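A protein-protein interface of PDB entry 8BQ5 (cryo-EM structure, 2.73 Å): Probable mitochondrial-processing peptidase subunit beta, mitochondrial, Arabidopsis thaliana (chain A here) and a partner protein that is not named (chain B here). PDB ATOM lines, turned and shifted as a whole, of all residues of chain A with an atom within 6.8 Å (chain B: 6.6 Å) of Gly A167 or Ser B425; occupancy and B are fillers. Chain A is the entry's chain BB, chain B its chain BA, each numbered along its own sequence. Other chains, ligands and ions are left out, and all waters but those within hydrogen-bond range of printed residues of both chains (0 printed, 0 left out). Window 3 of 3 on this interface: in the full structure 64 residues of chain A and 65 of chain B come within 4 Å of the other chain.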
ATOM      1  N   THR A 118      14.261  10.592 -22.176  1.00  0.00           N
ATOM      2  CA  THR A 118      15.273  11.398 -21.513  1.00  0.00           C
ATOM      3  C   THR A 118      15.135  12.858 -21.925  1.00  0.00           C
ATOM      4  O   THR A 118      14.287  13.224 -22.742  1.00  0.00           O
ATOM      5  CB  THR A 118      16.685  10.895 -21.837  1.00  0.00           C
ATOM      6  OG1 THR A 118      16.818  10.728 -23.254  1.00  0.00           O
ATOM      7  CG2 THR A 118      16.945   9.568 -21.147  1.00  0.00           C
ATOM      8  N   GLU A 162      22.662  13.323  -4.841  1.00  0.00           N
ATOM      9  CA  GLU A 162      21.386  13.595  -5.493  1.00  0.00           C
ATOM     10  C   GLU A 162      21.456  13.353  -6.996  1.00  0.00           C
ATOM     11  O   GLU A 162      20.484  12.871  -7.591  1.00  0.00           O
ATOM     12  CB  GLU A 162      20.938  15.025  -5.186  1.00  0.00           C
ATOM     13  CG  GLU A 162      20.010  15.635  -6.217  1.00  0.00           C
ATOM     14  CD  GLU A 162      19.808  17.118  -6.001  1.00  0.00           C
ATOM     15  OE1 GLU A 162      20.778  17.800  -5.616  1.00  0.00           O
ATOM     16  OE2 GLU A 162      18.675  17.600  -6.212  1.00  0.00           O
ATOM     17  N   ILE A 163      22.590  13.667  -7.626  1.00  0.00           N
ATOM     18  CA  ILE A 163      22.726  13.431  -9.061  1.00  0.00           C
ATOM     19  C   ILE A 163      22.769  11.936  -9.359  1.00  0.00           C
ATOM     20  O   ILE A 163      22.134  11.460 -10.309  1.00  0.00           O
ATOM     21  CB  ILE A 163      23.967  14.161  -9.609  1.00  0.00           C
ATOM     22  CG1 ILE A 163      23.776  15.676  -9.504  1.00  0.00           C
ATOM     23  CG2 ILE A 163      24.239  13.759 -11.048  1.00  0.00           C
ATOM     24  CD1 ILE A 163      22.723  16.225 -10.438  1.00  0.00           C
ATOM     25  N   GLU A 164      23.508  11.170  -8.553  1.00  0.00           N
ATOM     26  CA  GLU A 164      23.603   9.734  -8.803  1.00  0.00           C
ATOM     27  C   GLU A 164      22.330   8.999  -8.404  1.00  0.00           C
ATOM     28  O   GLU A 164      22.079   7.893  -8.898  1.00  0.00           O
ATOM     29  CB  GLU A 164      24.810   9.143  -8.071  1.00  0.00           C
ATOM     30  CG  GLU A 164      26.148   9.696  -8.532  1.00  0.00           C
ATOM     31  CD  GLU A 164      27.201   9.671  -7.441  1.00  0.00           C
ATOM     32  OE1 GLU A 164      26.871   9.280  -6.302  1.00  0.00           O
ATOM     33  OE2 GLU A 164      28.360  10.037  -7.725  1.00  0.00           O
ATOM     34  N   ASP A 165      21.518   9.584  -7.521  1.00  0.00           N
ATOM     35  CA  ASP A 165      20.270   8.933  -7.132  1.00  0.00           C
ATOM     36  C   ASP A 165      19.271   8.908  -8.281  1.00  0.00           C
ATOM     37  O   ASP A 165      18.510   7.944  -8.427  1.00  0.00           O
ATOM     38  CB  ASP A 165      19.669   9.625  -5.909  1.00  0.00           C
ATOM     39  CG  ASP A 165      20.463   9.364  -4.645  1.00  0.00           C
ATOM     40  OD1 ASP A 165      21.298   8.436  -4.651  1.00  0.00           O
ATOM     41  OD2 ASP A 165      20.264  10.090  -3.649  1.00  0.00           O
ATOM     42  N   ILE A 166      19.249   9.960  -9.105  1.00  0.00           N
ATOM     43  CA  ILE A 166      18.369   9.971 -10.272  1.00  0.00           C
ATOM     44  C   ILE A 166      19.063   9.482 -11.530  1.00  0.00           C
ATOM     45  O   ILE A 166      18.458   9.511 -12.609  1.00  0.00           O
ATOM     46  CB  ILE A 166      17.805  11.378 -10.549  1.00  0.00           C
ATOM     47  CG1 ILE A 166      18.929  12.414 -10.554  1.00  0.00           C
ATOM     48  CG2 ILE A 166      16.738  11.735  -9.527  1.00  0.00           C
ATOM     49  CD1 ILE A 166      18.457  13.820 -10.833  1.00  0.00           C
ATOM     50  N   GLY A 167      20.311   9.032 -11.423  1.00  0.00           N
ATOM     51  CA  GLY A 167      21.056   8.602 -12.585  1.00  0.00           C
ATOM     52  C   GLY A 167      21.320   9.685 -13.602  1.00  0.00           C
ATOM     53  O   GLY A 167      21.369   9.395 -14.802  1.00  0.00           O
ATOM     54  N   GLY A 168      21.491  10.929 -13.162  1.00  0.00           N
ATOM     55  CA  GLY A 168      21.763  12.034 -14.055  1.00  0.00           C
ATOM     56  C   GLY A 168      23.246  12.226 -14.302  1.00  0.00           C
ATOM     57  O   GLY A 168      24.101  11.510 -13.776  1.00  0.00           O
ATOM     58  N   HIS A 169      23.549  13.223 -15.131  1.00  0.00           N
ATOM     59  CA  HIS A 169      24.916  13.577 -15.475  1.00  0.00           C
ATOM     60  C   HIS A 169      25.054  15.089 -15.435  1.00  0.00           C
ATOM     61  O   HIS A 169      24.159  15.809 -15.883  1.00  0.00           O
ATOM     62  CB  HIS A 169      25.298  13.059 -16.869  1.00  0.00           C
ATOM     63  CG  HIS A 169      25.367  11.567 -16.965  1.00  0.00           C
ATOM     64  ND1 HIS A 169      26.457  10.843 -16.532  1.00  0.00           N
ATOM     65  CD2 HIS A 169      24.485  10.663 -17.453  1.00  0.00           C
ATOM     66  CE1 HIS A 169      26.241   9.557 -16.746  1.00  0.00           C
ATOM     67  NE2 HIS A 169      25.051   9.421 -17.303  1.00  0.00           N
ATOM     68  N   LYS A 184      22.121  15.908 -18.070  1.00  0.00           N
ATOM     69  CA  LYS A 184      21.413  14.857 -18.794  1.00  0.00           C
ATOM     70  C   LYS A 184      20.652  14.021 -17.774  1.00  0.00           C
ATOM     71  O   LYS A 184      21.261  13.340 -16.943  1.00  0.00           O
ATOM     72  CB  LYS A 184      22.380  13.993 -19.599  1.00  0.00           C
ATOM     73  CG  LYS A 184      23.015  14.700 -20.779  1.00  0.00           C
ATOM     74  CD  LYS A 184      24.082  13.834 -21.425  1.00  0.00           C
ATOM     75  CE  LYS A 184      23.507  12.508 -21.891  1.00  0.00           C
ATOM     76  NZ  LYS A 184      22.259  12.687 -22.681  1.00  0.00           N
ATOM     77  N   VAL A 185      19.322  14.074 -17.831  1.00  0.00           N
ATOM     78  CA  VAL A 185      18.465  13.432 -16.843  1.00  0.00           C
ATOM     79  C   VAL A 185      17.307  12.748 -17.557  1.00  0.00           C
ATOM     80  O   VAL A 185      17.083  12.933 -18.754  1.00  0.00           O
ATOM     81  CB  VAL A 185      17.929  14.434 -15.799  1.00  0.00           C
ATOM     82  CG1 VAL A 185      19.067  14.997 -14.961  1.00  0.00           C
ATOM     83  CG2 VAL A 185      17.164  15.551 -16.485  1.00  0.00           C
ATOM     84  N   LEU A 186      16.568  11.944 -16.798  1.00  0.00           N
ATOM     85  CA  LEU A 186      15.359  11.323 -17.311  1.00  0.00           C
ATOM     86  C   LEU A 186      14.231  12.349 -17.397  1.00  0.00           C
ATOM     87  O   LEU A 186      14.303  13.443 -16.832  1.00  0.00           O
ATOM     88  CB  LEU A 186      14.941  10.149 -16.427  1.00  0.00           C
ATOM     89  CG  LEU A 186      16.032   9.139 -16.069  1.00  0.00           C
ATOM     90  CD1 LEU A 186      15.457   8.002 -15.245  1.00  0.00           C
ATOM     91  CD2 LEU A 186      16.704   8.603 -17.323  1.00  0.00           C
ATOM     92  N   ASN A 189      12.840  13.867 -14.180  1.00  0.00           N
ATOM     93  CA  ASN A 189      13.739  14.620 -13.311  1.00  0.00           C
ATOM     94  C   ASN A 189      14.153  15.952 -13.927  1.00  0.00           C
ATOM     95  O   ASN A 189      15.187  16.508 -13.547  1.00  0.00           O
ATOM     96  CB  ASN A 189      14.976  13.787 -12.972  1.00  0.00           C
ATOM     97  CG  ASN A 189      14.624  12.408 -12.453  1.00  0.00           C
ATOM     98  OD1 ASN A 189      15.125  11.400 -12.951  1.00  0.00           O
ATOM     99  ND2 ASN A 189      13.752  12.357 -11.455  1.00  0.00           N
ATOM    100  N   MET B 333      28.099  -1.656 -12.915  1.00  0.00           N
ATOM    101  CA  MET B 333      27.838  -0.281 -12.512  1.00  0.00           C
ATOM    102  C   MET B 333      28.016  -0.080 -11.014  1.00  0.00           C
ATOM    103  O   MET B 333      28.254   1.052 -10.577  1.00  0.00           O
ATOM    104  CB  MET B 333      26.427   0.126 -12.934  1.00  0.00           C
ATOM    105  CG  MET B 333      26.235   0.187 -14.436  1.00  0.00           C
ATOM    106  SD  MET B 333      27.345   1.377 -15.213  1.00  0.00           S
ATOM    107  CE  MET B 333      26.708   2.916 -14.555  1.00  0.00           C
ATOM    108  N   ARG B 418      21.587   3.542  -6.494  1.00  0.00           N
ATOM    109  CA  ARG B 418      22.338   4.391  -7.412  1.00  0.00           C
ATOM    110  C   ARG B 418      22.845   3.594  -8.605  1.00  0.00           C
ATOM    111  O   ARG B 418      22.816   4.077  -9.743  1.00  0.00           O
ATOM    112  CB  ARG B 418      23.493   5.068  -6.677  1.00  0.00           C
ATOM    113  CG  ARG B 418      23.036   6.167  -5.739  1.00  0.00           C
ATOM    114  CD  ARG B 418      24.196   6.993  -5.218  1.00  0.00           C
ATOM    115  NE  ARG B 418      24.935   6.308  -4.166  1.00  0.00           N
ATOM    116  CZ  ARG B 418      24.971   6.703  -2.902  1.00  0.00           C
ATOM    117  NH1 ARG B 418      24.264   7.739  -2.484  1.00  0.00           N
ATOM    118  NH2 ARG B 418      25.728   6.038  -2.035  1.00  0.00           N
ATOM    119  N   LYS B 420      21.353   0.974  -9.751  1.00  0.00           N
ATOM    120  CA  LYS B 420      20.151   0.701 -10.533  1.00  0.00           C
ATOM    121  C   LYS B 420      19.803   1.881 -11.432  1.00  0.00           C
ATOM    122  O   LYS B 420      19.503   1.708 -12.618  1.00  0.00           O
ATOM    123  CB  LYS B 420      18.983   0.383  -9.603  1.00  0.00           C
ATOM    124  CG  LYS B 420      18.984  -1.018  -9.037  1.00  0.00           C
ATOM    125  CD  LYS B 420      17.794  -1.202  -8.117  1.00  0.00           C
ATOM    126  CE  LYS B 420      17.731  -2.606  -7.558  1.00  0.00           C
ATOM    127  NZ  LYS B 420      16.364  -2.921  -7.062  1.00  0.00           N
ATOM    128  N   ALA B 421      19.829   3.094 -10.873  1.00  0.00           N
ATOM    129  CA  ALA B 421      19.494   4.279 -11.654  1.00  0.00           C
ATOM    130  C   ALA B 421      20.535   4.544 -12.732  1.00  0.00           C
ATOM    131  O   ALA B 421      20.197   4.973 -13.841  1.00  0.00           O
ATOM    132  CB  ALA B 421      19.353   5.491 -10.733  1.00  0.00           C
ATOM    133  N   ALA B 422      21.811   4.304 -12.421  1.00  0.00           N
ATOM    134  CA  ALA B 422      22.856   4.469 -13.425  1.00  0.00           C
ATOM    135  C   ALA B 422      22.679   3.476 -14.566  1.00  0.00           C
ATOM    136  O   ALA B 422      22.889   3.819 -15.734  1.00  0.00           O
ATOM    137  CB  ALA B 422      24.232   4.313 -12.780  1.00  0.00           C
ATOM    138  N   THR B 423      22.300   2.238 -14.244  1.00  0.00           N
ATOM    139  CA  THR B 423      22.059   1.241 -15.283  1.00  0.00           C
ATOM    140  C   THR B 423      20.861   1.623 -16.145  1.00  0.00           C
ATOM    141  O   THR B 423      20.923   1.563 -17.378  1.00  0.00           O
ATOM    142  CB  THR B 423      21.849  -0.135 -14.649  1.00  0.00           C
ATOM    143  OG1 THR B 423      23.118  -0.689 -14.278  1.00  0.00           O
ATOM    144  CG2 THR B 423      21.158  -1.077 -15.622  1.00  0.00           C
ATOM    145  N   LYS B 424      19.758   2.027 -15.508  1.00  0.00           N
ATOM    146  CA  LYS B 424      18.544   2.335 -16.257  1.00  0.00           C
ATOM    147  C   LYS B 424      18.732   3.566 -17.137  1.00  0.00           C
ATOM    148  O   LYS B 424      18.273   3.593 -18.285  1.00  0.00           O
ATOM    149  CB  LYS B 424      17.370   2.524 -15.296  1.00  0.00           C
ATOM    150  CG  LYS B 424      16.332   3.533 -15.755  1.00  0.00           C
ATOM    151  CD  LYS B 424      15.103   3.502 -14.861  1.00  0.00           C
ATOM    152  CE  LYS B 424      13.850   3.880 -15.632  1.00  0.00           C
ATOM    153  NZ  LYS B 424      12.851   4.577 -14.777  1.00  0.00           N
ATOM    154  N   SER B 425      19.405   4.595 -16.616  1.00  0.00           N
ATOM    155  CA  SER B 425      19.654   5.788 -17.418  1.00  0.00           C
ATOM    156  C   SER B 425      20.582   5.494 -18.589  1.00  0.00           C
ATOM    157  O   SER B 425      20.361   6.006 -19.692  1.00  0.00           O
ATOM    158  CB  SER B 425      20.245   6.900 -16.552  1.00  0.00           C
ATOM    159  OG  SER B 425      21.545   6.559 -16.108  1.00  0.00           O
ATOM    160  N   ALA B 426      21.617   4.680 -18.370  1.00  0.00           N
ATOM    161  CA  ALA B 426      22.576   4.384 -19.430  1.00  0.00           C
ATOM    162  C   ALA B 426      21.915   3.684 -20.610  1.00  0.00           C
ATOM    163  O   ALA B 426      22.182   4.030 -21.764  1.00  0.00           O
ATOM    164  CB  ALA B 426      23.721   3.534 -18.882  1.00  0.00           C
ATOM    165  N   VAL B 427      21.051   2.705 -20.343  1.00  0.00           N
ATOM    166  CA  VAL B 427      20.372   2.002 -21.427  1.00  0.00           C
ATOM    167  C   VAL B 427      19.481   2.960 -22.207  1.00  0.00           C
ATOM    168  O   VAL B 427      19.473   2.963 -23.444  1.00  0.00           O
ATOM    169  CB  VAL B 427      19.574   0.810 -20.872  1.00  0.00           C
ATOM    170  CG1 VAL B 427      18.583   0.304 -21.905  1.00  0.00           C
ATOM    171  CG2 VAL B 427      20.522  -0.298 -20.452  1.00  0.00           C
ATOM    172  N   LEU B 428      18.730   3.803 -21.496  1.00  0.00           N
ATOM    173  CA  LEU B 428      17.794   4.702 -22.160  1.00  0.00           C
ATOM    174  C   LEU B 428      18.518   5.834 -22.879  1.00  0.00           C
ATOM    175  O   LEU B 428      18.004   6.384 -23.860  1.00  0.00           O
ATOM    176  CB  LEU B 428      16.802   5.262 -21.140  1.00  0.00           C
ATOM    177  CG  LEU B 428      15.647   4.343 -20.745  1.00  0.00           C
ATOM    178  CD1 LEU B 428      14.753   5.020 -19.720  1.00  0.00           C
ATOM    179  CD2 LEU B 428      14.845   3.941 -21.971  1.00  0.00           C
ATOM    180  N   MET B 429      19.712   6.202 -22.406  1.00  0.00           N
ATOM    181  CA  MET B 429      20.393   7.367 -22.961  1.00  0.00           C
ATOM    182  C   MET B 429      21.096   7.036 -24.273  1.00  0.00           C
ATOM    183  O   MET B 429      21.093   7.844 -25.208  1.00  0.00           O
ATOM    184  CB  MET B 429      21.382   7.934 -21.945  1.00  0.00           C
ATOM    185  CG  MET B 429      20.813   9.079 -21.125  1.00  0.00           C
ATOM    186  SD  MET B 429      21.732   9.387 -19.609  1.00  0.00           S
ATOM    187  CE  MET B 429      20.573  10.429 -18.726  1.00  0.00           C
ATOM    188  N   ASN B 430      21.710   5.853 -24.365  1.00  0.00           N
ATOM    189  CA  ASN B 430      22.340   5.463 -25.623  1.00  0.00           C
ATOM    190  C   ASN B 430      21.299   5.201 -26.700  1.00  0.00           C
ATOM    191  O   ASN B 430      21.604   5.250 -27.897  1.00  0.00           O
ATOM    192  CB  ASN B 430      23.218   4.227 -25.427  1.00  0.00           C
ATOM    193  CG  ASN B 430      24.471   4.519 -24.638  1.00  0.00           C
ATOM    194  OD1 ASN B 430      24.929   5.659 -24.579  1.00  0.00           O
ATOM    195  ND2 ASN B 430      25.035   3.486 -24.024  1.00  0.00           N
ATOM    196  N   LEU B 458      14.002  -2.985 -17.917  1.00  0.00           N
ATOM    197  CA  LEU B 458      13.993  -2.076 -16.776  1.00  0.00           C
ATOM    198  C   LEU B 458      13.284  -2.694 -15.579  1.00  0.00           C
ATOM    199  O   LEU B 458      13.674  -2.455 -14.431  1.00  0.00           O
ATOM    200  CB  LEU B 458      13.337  -0.753 -17.171  1.00  0.00           C
ATOM    201  CG  LEU B 458      14.063   0.059 -18.248  1.00  0.00           C
ATOM    202  CD1 LEU B 458      13.536   1.481 -18.292  1.00  0.00           C
ATOM    203  CD2 LEU B 458      15.566   0.054 -18.011  1.00  0.00           C
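The guanidinium group of Arg B418 is in salt-bridge range of the side-chain carboxylate of Asp A165. OG of Ser B425 sits at hydrogen-bond distance from O of Gly A167 (3.1 Å).
The side-chain hydroxyl of Ser B425 is in hydrogen-bond range of the backbone carbonyl oxygen of Ala B421 (3.1 Å). O of Ala B422 sits at hydrogen-bond distance from OG of Ser B425 (3.1 Å). The backbone carbonyl oxygen of Lys A184 sits at hydrogen-bond distance from the backbone NH of His A169 (2.9 Å).
Among the printed residues, pairs that only touch across the chains: Asp A165 with Ala B421 (3.5 Å), Lys A184 with Met B429 (3.5 Å), Glu A164 with Arg B418 (3.6 Å), His A169 with Met B429 (3.7 Å), Gly A167 with Ala B421 (3.7 Å), Thr A118 with Met B429 (3.9 Å) and Val A185 with Met B429 (3.96 Å).
Gly A167 touches just these residues of chain B: Ala B421 (3.7 Å) and Ser B425 (3.1 Å). Of the printed residues of chain A, Ser B425 touches Gly A167. Of the printed residues of chain A, Arg B418 touches Glu A164 and Asp A165. Of the printed residues of chain A, Ala B421 touches Asp A165 (3.5 Å) and Gly A167 (3.7 Å). Of the printed residues of chain B, Lys A184 touches Met B429 (3.5 Å). Met B333 touches none of the printed residues of chain A. Leu B458 touches none of the printed residues of chain A.
Of the 13 printed residues of chain A, 7 touch a printed residue of chain B. Printed residues of chain B that touch a printed residue of chain A: Arg B418, Ala B421, Ser B425 and Met B429. Among the printed residues, Asp or Glu carboxylates within 4 Å of a Lys or Arg side-chain nitrogen of the other chain: Asp A165 with Arg B418.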
